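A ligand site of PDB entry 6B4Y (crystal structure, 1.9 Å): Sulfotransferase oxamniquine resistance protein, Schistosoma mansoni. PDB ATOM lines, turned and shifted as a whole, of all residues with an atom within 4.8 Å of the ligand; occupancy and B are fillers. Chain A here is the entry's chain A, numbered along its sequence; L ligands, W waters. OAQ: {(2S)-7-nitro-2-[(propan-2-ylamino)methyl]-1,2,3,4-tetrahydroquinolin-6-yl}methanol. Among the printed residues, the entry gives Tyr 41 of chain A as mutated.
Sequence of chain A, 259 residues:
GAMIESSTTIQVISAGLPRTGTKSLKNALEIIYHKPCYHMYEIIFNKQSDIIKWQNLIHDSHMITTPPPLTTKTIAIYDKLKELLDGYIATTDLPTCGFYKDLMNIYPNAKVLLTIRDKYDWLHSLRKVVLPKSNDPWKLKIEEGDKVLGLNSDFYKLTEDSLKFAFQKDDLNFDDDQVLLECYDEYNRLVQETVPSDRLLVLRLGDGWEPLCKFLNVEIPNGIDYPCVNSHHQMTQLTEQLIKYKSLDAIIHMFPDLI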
ATOM      1  N   PRO A  18     -35.144  33.100  12.302  1.00  0.00           N
ATOM      2  CA  PRO A  18     -34.234  31.966  12.185  1.00  0.00           C
ATOM      3  C   PRO A  18     -34.551  31.085  10.958  1.00  0.00           C
ATOM      4  O   PRO A  18     -35.706  31.024  10.551  1.00  0.00           O
ATOM      5  CB  PRO A  18     -34.470  31.183  13.481  1.00  0.00           C
ATOM      6  CG  PRO A  18     -35.707  31.766  14.075  1.00  0.00           C
ATOM      7  CD  PRO A  18     -35.762  33.174  13.641  1.00  0.00           C
ATOM      8  N   HIS A  39     -25.709  36.679  17.239  1.00  0.00           N
ATOM      9  CA  HIS A  39     -26.437  35.565  16.628  1.00  0.00           C
ATOM     10  C   HIS A  39     -26.761  34.592  17.761  1.00  0.00           C
ATOM     11  O   HIS A  39     -26.133  34.681  18.788  1.00  0.00           O
ATOM     12  CB  HIS A  39     -25.592  34.865  15.573  1.00  0.00           C
ATOM     13  CG  HIS A  39     -26.337  33.859  14.750  1.00  0.00           C
ATOM     14  ND1 HIS A  39     -26.464  32.537  15.125  1.00  0.00           N
ATOM     15  CD2 HIS A  39     -27.006  33.987  13.591  1.00  0.00           C
ATOM     16  CE1 HIS A  39     -27.173  31.888  14.216  1.00  0.00           C
ATOM     17  NE2 HIS A  39     -27.507  32.747  13.274  1.00  0.00           N
ATOM     18  N   MET A  40     -27.707  33.675  17.583  1.00  0.00           N
ATOM     19  CA  MET A  40     -27.901  32.677  18.628  1.00  0.00           C
ATOM     20  C   MET A  40     -26.609  31.880  18.850  1.00  0.00           C
ATOM     21  O   MET A  40     -26.308  31.495  19.965  1.00  0.00           O
ATOM     22  CB  MET A  40     -29.075  31.745  18.300  1.00  0.00           C
ATOM     23  CG  MET A  40     -29.455  30.753  19.416  1.00  0.00           C
ATOM     24  SD  MET A  40     -29.967  31.550  20.973  1.00  0.00           S
ATOM     25  CE  MET A  40     -31.691  31.927  20.683  1.00  0.00           C
ATOM     26  N   TYR A  41     -25.829  31.666  17.796  1.00  0.00           N
ATOM     27  CA  TYR A  41     -24.540  30.965  17.928  1.00  0.00           C
ATOM     28  C   TYR A  41     -23.620  31.639  18.936  1.00  0.00           C
ATOM     29  O   TYR A  41     -22.865  30.974  19.636  1.00  0.00           O
ATOM     30  CB  TYR A  41     -23.828  30.896  16.588  1.00  0.00           C
ATOM     31  CG  TYR A  41     -24.227  29.710  15.733  1.00  0.00           C
ATOM     32  CD1 TYR A  41     -25.555  29.479  15.435  1.00  0.00           C
ATOM     33  CD2 TYR A  41     -23.274  28.848  15.228  1.00  0.00           C
ATOM     34  CE1 TYR A  41     -25.916  28.404  14.649  1.00  0.00           C
ATOM     35  CE2 TYR A  41     -23.635  27.774  14.442  1.00  0.00           C
ATOM     36  CZ  TYR A  41     -24.948  27.560  14.152  1.00  0.00           C
ATOM     37  OH  TYR A  41     -25.309  26.485  13.366  1.00  0.00           O
ATOM     38  N   ILE A  44     -24.883  30.525  22.335  1.00  0.00           N
ATOM     39  CA  ILE A  44     -24.617  29.115  22.598  1.00  0.00           C
ATOM     40  C   ILE A  44     -23.146  28.832  22.828  1.00  0.00           C
ATOM     41  O   ILE A  44     -22.777  28.141  23.773  1.00  0.00           O
ATOM     42  CB  ILE A  44     -25.102  28.234  21.441  1.00  0.00           C
ATOM     43  CG1 ILE A  44     -26.626  28.293  21.324  1.00  0.00           C
ATOM     44  CG2 ILE A  44     -24.635  26.795  21.637  1.00  0.00           C
ATOM     45  CD1 ILE A  44     -27.140  27.638  20.053  1.00  0.00           C
ATOM     46  N   ASP A  93     -30.890  37.107  13.938  1.00  0.00           N
ATOM     47  CA  ASP A  93     -31.467  35.911  14.561  1.00  0.00           C
ATOM     48  C   ASP A  93     -32.144  36.191  15.920  1.00  0.00           C
ATOM     49  O   ASP A  93     -32.058  37.295  16.461  1.00  0.00           O
ATOM     50  CB  ASP A  93     -30.354  34.864  14.717  1.00  0.00           C
ATOM     51  CG  ASP A  93     -30.871  33.471  14.989  1.00  0.00           C
ATOM     52  OD1 ASP A  93     -32.026  33.145  14.640  1.00  0.00           O
ATOM     53  OD2 ASP A  93     -30.084  32.678  15.542  1.00  0.00           O
ATOM     54  N   LEU A  94     -32.824  35.181  16.464  1.00  0.00           N
ATOM     55  CA  LEU A  94     -33.304  35.233  17.846  1.00  0.00           C
ATOM     56  C   LEU A  94     -32.094  35.320  18.772  1.00  0.00           C
ATOM     57  O   LEU A  94     -31.020  34.847  18.418  1.00  0.00           O
ATOM     58  CB  LEU A  94     -34.150  34.006  18.170  1.00  0.00           C
ATOM     59  CG  LEU A  94     -35.419  33.749  17.362  1.00  0.00           C
ATOM     60  CD1 LEU A  94     -35.975  32.371  17.682  1.00  0.00           C
ATOM     61  CD2 LEU A  94     -36.465  34.824  17.665  1.00  0.00           C
ATOM     62  N   VAL A 129     -34.395  21.753  13.098  1.00  0.00           N
ATOM     63  CA  VAL A 129     -33.327  22.373  13.860  1.00  0.00           C
ATOM     64  C   VAL A 129     -33.809  23.058  15.117  1.00  0.00           C
ATOM     65  O   VAL A 129     -33.272  22.854  16.193  1.00  0.00           O
ATOM     66  CB  VAL A 129     -32.581  23.405  12.992  1.00  0.00           C
ATOM     67  CG1 VAL A 129     -31.520  24.158  13.821  1.00  0.00           C
ATOM     68  CG2 VAL A 129     -31.943  22.723  11.775  1.00  0.00           C
ATOM     69  N   VAL A 130     -34.834  23.893  14.962  1.00  0.00           N
ATOM     70  CA  VAL A 130     -35.212  24.831  16.013  1.00  0.00           C
ATOM     71  C   VAL A 130     -36.420  24.385  16.802  1.00  0.00           C
ATOM     72  O   VAL A 130     -36.440  24.474  18.039  1.00  0.00           O
ATOM     73  CB  VAL A 130     -35.529  26.210  15.411  1.00  0.00           C
ATOM     74  CG1 VAL A 130     -35.859  27.211  16.496  1.00  0.00           C
ATOM     75  CG2 VAL A 130     -34.361  26.694  14.588  1.00  0.00           C
ATOM     76  N   ILE A 142     -32.094  15.996  19.290  1.00  0.00           N
ATOM     77  CA  ILE A 142     -31.762  17.405  19.489  1.00  0.00           C
ATOM     78  C   ILE A 142     -31.505  17.704  20.977  1.00  0.00           C
ATOM     79  O   ILE A 142     -30.545  18.384  21.320  1.00  0.00           O
ATOM     80  CB  ILE A 142     -32.882  18.313  18.975  1.00  0.00           C
ATOM     81  CG1 ILE A 142     -32.982  18.207  17.448  1.00  0.00           C
ATOM     82  CG2 ILE A 142     -32.642  19.749  19.403  1.00  0.00           C
ATOM     83  CD1 ILE A 142     -34.152  18.999  16.885  1.00  0.00           C
ATOM     84  N   GLY A 145     -28.169  16.094  22.156  1.00  0.00           N
ATOM     85  CA  GLY A 145     -27.051  16.885  21.654  1.00  0.00           C
ATOM     86  C   GLY A 145     -26.897  18.226  22.353  1.00  0.00           C
ATOM     87  O   GLY A 145     -25.783  18.661  22.651  1.00  0.00           O
ATOM     88  N   ASP A 146     -28.008  18.898  22.616  1.00  0.00           N
ATOM     89  CA  ASP A 146     -27.970  20.186  23.310  1.00  0.00           C
ATOM     90  C   ASP A 146     -27.398  20.070  24.729  1.00  0.00           C
ATOM     91  O   ASP A 146     -26.749  20.993  25.199  1.00  0.00           O
ATOM     92  CB  ASP A 146     -29.370  20.801  23.358  1.00  0.00           C
ATOM     93  CG  ASP A 146     -29.802  21.409  22.040  1.00  0.00           C
ATOM     94  OD1 ASP A 146     -28.924  21.700  21.196  1.00  0.00           O
ATOM     95  OD2 ASP A 146     -31.016  21.615  21.838  1.00  0.00           O
ATOM     96  N   LEU A 149     -23.741  20.381  24.759  1.00  0.00           N
ATOM     97  CA  LEU A 149     -23.312  21.773  24.648  1.00  0.00           C
ATOM     98  C   LEU A 149     -23.509  22.562  25.945  1.00  0.00           C
ATOM     99  O   LEU A 149     -23.063  23.692  26.062  1.00  0.00           O
ATOM    100  CB  LEU A 149     -24.075  22.481  23.521  1.00  0.00           C
ATOM    101  CG  LEU A 149     -23.902  21.976  22.084  1.00  0.00           C
ATOM    102  CD1 LEU A 149     -24.728  22.811  21.115  1.00  0.00           C
ATOM    103  CD2 LEU A 149     -22.428  22.028  21.718  1.00  0.00           C
ATOM    104  N   PHE A 155     -32.590  27.441  27.962  1.00  0.00           N
ATOM    105  CA  PHE A 155     -32.304  27.786  26.580  1.00  0.00           C
ATOM    106  C   PHE A 155     -33.546  27.587  25.705  1.00  0.00           C
ATOM    107  O   PHE A 155     -33.848  28.417  24.867  1.00  0.00           O
ATOM    108  CB  PHE A 155     -31.138  26.946  26.042  1.00  0.00           C
ATOM    109  CG  PHE A 155     -30.953  27.057  24.553  1.00  0.00           C
ATOM    110  CD1 PHE A 155     -30.300  28.156  23.990  1.00  0.00           C
ATOM    111  CD2 PHE A 155     -31.433  26.071  23.708  1.00  0.00           C
ATOM    112  CE1 PHE A 155     -30.133  28.253  22.623  1.00  0.00           C
ATOM    113  CE2 PHE A 155     -31.263  26.177  22.331  1.00  0.00           C
ATOM    114  CZ  PHE A 155     -30.615  27.260  21.799  1.00  0.00           C
ATOM    115  N   THR A 159     -35.769  30.459  23.524  1.00  0.00           N
ATOM    116  CA  THR A 159     -36.171  30.322  22.121  1.00  0.00           C
ATOM    117  C   THR A 159     -37.675  30.564  21.915  1.00  0.00           C
ATOM    118  O   THR A 159     -38.083  31.350  21.072  1.00  0.00           O
ATOM    119  CB  THR A 159     -35.803  28.939  21.587  1.00  0.00           C
ATOM    120  OG1 THR A 159     -34.378  28.773  21.615  1.00  0.00           O
ATOM    121  CG2 THR A 159     -36.315  28.777  20.146  1.00  0.00           C
ATOM    122  N   ASN A 230     -24.884  26.380   7.808  1.00  0.00           N
ATOM    123  CA  ASN A 230     -25.976  26.191   8.772  1.00  0.00           C
ATOM    124  C   ASN A 230     -27.229  25.554   8.163  1.00  0.00           C
ATOM    125  O   ASN A 230     -28.343  25.808   8.609  1.00  0.00           O
ATOM    126  CB  ASN A 230     -26.355  27.548   9.428  1.00  0.00           C
ATOM    127  CG  ASN A 230     -26.897  27.369  10.833  1.00  0.00           C
ATOM    128  OD1 ASN A 230     -26.575  26.401  11.504  1.00  0.00           O
ATOM    129  ND2 ASN A 230     -27.737  28.298  11.282  1.00  0.00           N
ATOM    130  N   MET A 235     -26.630  20.538  10.419  1.00  0.00           N
ATOM    131  CA  MET A 235     -27.031  20.539  11.816  1.00  0.00           C
ATOM    132  C   MET A 235     -27.401  19.137  12.300  1.00  0.00           C
ATOM    133  O   MET A 235     -27.191  18.802  13.469  1.00  0.00           O
ATOM    134  CB  MET A 235     -28.197  21.503  12.040  1.00  0.00           C
ATOM    135  CG  MET A 235     -27.836  22.972  11.781  1.00  0.00           C
ATOM    136  SD  MET A 235     -26.278  23.492  12.563  1.00  0.00           S
ATOM    137  CE  MET A 235     -26.632  23.199  14.281  1.00  0.00           C
ATOM    138  N   LEU A 238     -24.057  17.573  12.921  1.00  0.00           N
ATOM    139  CA  LEU A 238     -23.502  18.071  14.188  1.00  0.00           C
ATOM    140  C   LEU A 238     -24.163  17.392  15.382  1.00  0.00           C
ATOM    141  O   LEU A 238     -23.499  16.951  16.301  1.00  0.00           O
ATOM    142  CB  LEU A 238     -23.637  19.586  14.296  1.00  0.00           C
ATOM    143  CG  LEU A 238     -23.251  20.231  15.638  1.00  0.00           C
ATOM    144  CD1 LEU A 238     -21.786  20.010  15.942  1.00  0.00           C
ATOM    145  CD2 LEU A 238     -23.568  21.710  15.608  1.00  0.00           C
ATOM    146  N   THR A 239     -25.486  17.323  15.358  1.00  0.00           N
ATOM    147  CA  THR A 239     -26.210  16.671  16.449  1.00  0.00           C
ATOM    148  C   THR A 239     -25.701  15.231  16.646  1.00  0.00           C
ATOM    149  O   THR A 239     -25.399  14.814  17.763  1.00  0.00           O
ATOM    150  CB  THR A 239     -27.715  16.669  16.188  1.00  0.00           C
ATOM    151  OG1 THR A 239     -28.155  18.014  15.951  1.00  0.00           O
ATOM    152  CG2 THR A 239     -28.464  16.087  17.382  1.00  0.00           C
ATOM    153  N   LEU A 242     -22.220  15.153  18.122  1.00  0.00           N
ATOM    154  CA  LEU A 242     -22.245  15.553  19.539  1.00  0.00           C
ATOM    155  C   LEU A 242     -22.638  14.374  20.422  1.00  0.00           C
ATOM    156  O   LEU A 242     -22.014  14.100  21.445  1.00  0.00           O
ATOM    157  CB  LEU A 242     -23.203  16.710  19.763  1.00  0.00           C
ATOM    158  CG  LEU A 242     -22.734  18.100  19.321  1.00  0.00           C
ATOM    159  CD1 LEU A 242     -23.890  19.092  19.441  1.00  0.00           C
ATOM    160  CD2 LEU A 242     -21.571  18.546  20.171  1.00  0.00           C
HETATM  161  C1  OAQ L   1     -30.166  28.035  16.052  1.00  0.00           C
HETATM  162  C2  OAQ L   1     -31.282  28.608  16.667  1.00  0.00           C
HETATM  163  C3  OAQ L   1     -31.875  27.898  17.724  1.00  0.00           C
HETATM  164  C4  OAQ L   1     -31.390  26.662  18.130  1.00  0.00           C
HETATM  165  C5  OAQ L   1     -30.278  26.109  17.503  1.00  0.00           C
HETATM  166  C6  OAQ L   1     -29.659  26.803  16.458  1.00  0.00           C
HETATM  167  C7  OAQ L   1     -28.592  24.309  17.314  1.00  0.00           C
HETATM  168  C8  OAQ L   1     -27.723  25.447  16.797  1.00  0.00           C
HETATM  169  C9  OAQ L   1     -28.539  26.278  15.818  1.00  0.00           C
HETATM  170  C10 OAQ L   1     -31.723  29.847  16.200  1.00  0.00           C
HETATM  171  C11 OAQ L   1     -27.813  23.414  18.279  1.00  0.00           C
HETATM  172  C12 OAQ L   1     -27.301  20.981  16.907  1.00  0.00           C
HETATM  173  C13 OAQ L   1     -28.580  19.717  18.673  1.00  0.00           C
HETATM  174  C14 OAQ L   1     -27.788  21.011  18.362  1.00  0.00           C
HETATM  175  N1  OAQ L   1     -29.796  24.868  17.961  1.00  0.00           N
HETATM  176  N2  OAQ L   1     -32.950  28.359  18.370  1.00  0.00           N
HETATM  177  N3  OAQ L   1     -28.601  22.216  18.621  1.00  0.00           N
HETATM  178  O1  OAQ L   1     -33.782  27.402  18.919  1.00  0.00           O
HETATM  179  O2  OAQ L   1     -33.191  29.876  18.619  1.00  0.00           O
HETATM  180  O3  OAQ L   1     -30.773  30.359  15.264  1.00  0.00           O
HETATM  181  O   HOH W   1     -30.688  21.665  16.425  1.00  0.00           O
HETATM  182  O   HOH W   2     -31.426  23.478  19.186  1.00  0.00           O
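O3 of the ligand sits at hydrogen-bond distance from OD2 of Asp 93. The side-chain carboxylate (OD1) of Asp 146 is in salt-bridge range of a nitrogen (N3) of the ligand (2.6 Å). The side-chain hydroxyl of Thr 159 lies within hydrogen-bond range of an oxygen (O1) of the ligand, 3.1 Å away.
The side-chain carboxylate (OD2) of Asp 93 lies close to the backbone NH (N) of Met 40. A ring nitrogen (NE2) of His 39 lies close to the side-chain carboxylate (OD2) of Asp 93. The backbone carbonyl oxygen of Phe 155 sits at hydrogen-bond distance from the side-chain hydroxyl of Thr 159, at 3.3 Å. OG1 of Thr 239 sits at hydrogen-bond distance from O of Met 235. The side-chain sulfur of Met 235 sits at hydrogen-bond distance from the side-chain hydroxyl of Tyr 41. OD1 of Asn 230 sits close to SD of Met 235, 3.1 Å away. A ring nitrogen (ND1) of His 39 is in hydrogen-bond range of the backbone NH (N) of Tyr 41.
Merely in contact with the ligand: Met 40, Tyr 41, Ile 44, Leu 94, Val 130, Ile 142, Phe 155, Met 235 and Thr 239. Hydrophobic or aromatic side chains that line the ligand: Met 40, Tyr 41, Ile 44, Leu 94, Val 130, Phe 155 and Met 235. Of the 20 residues printed, 12 come within 4 Å of the ligand.
Water W2 lies within hydrogen-bond range of a nitrogen (N1) of the ligand (2.5 Å) and the side-chain carboxylate (OD2) of Asp 146 (3.3 Å). Water W1 lies within hydrogen-bond range of O of Val 129 and N3 of the ligand.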
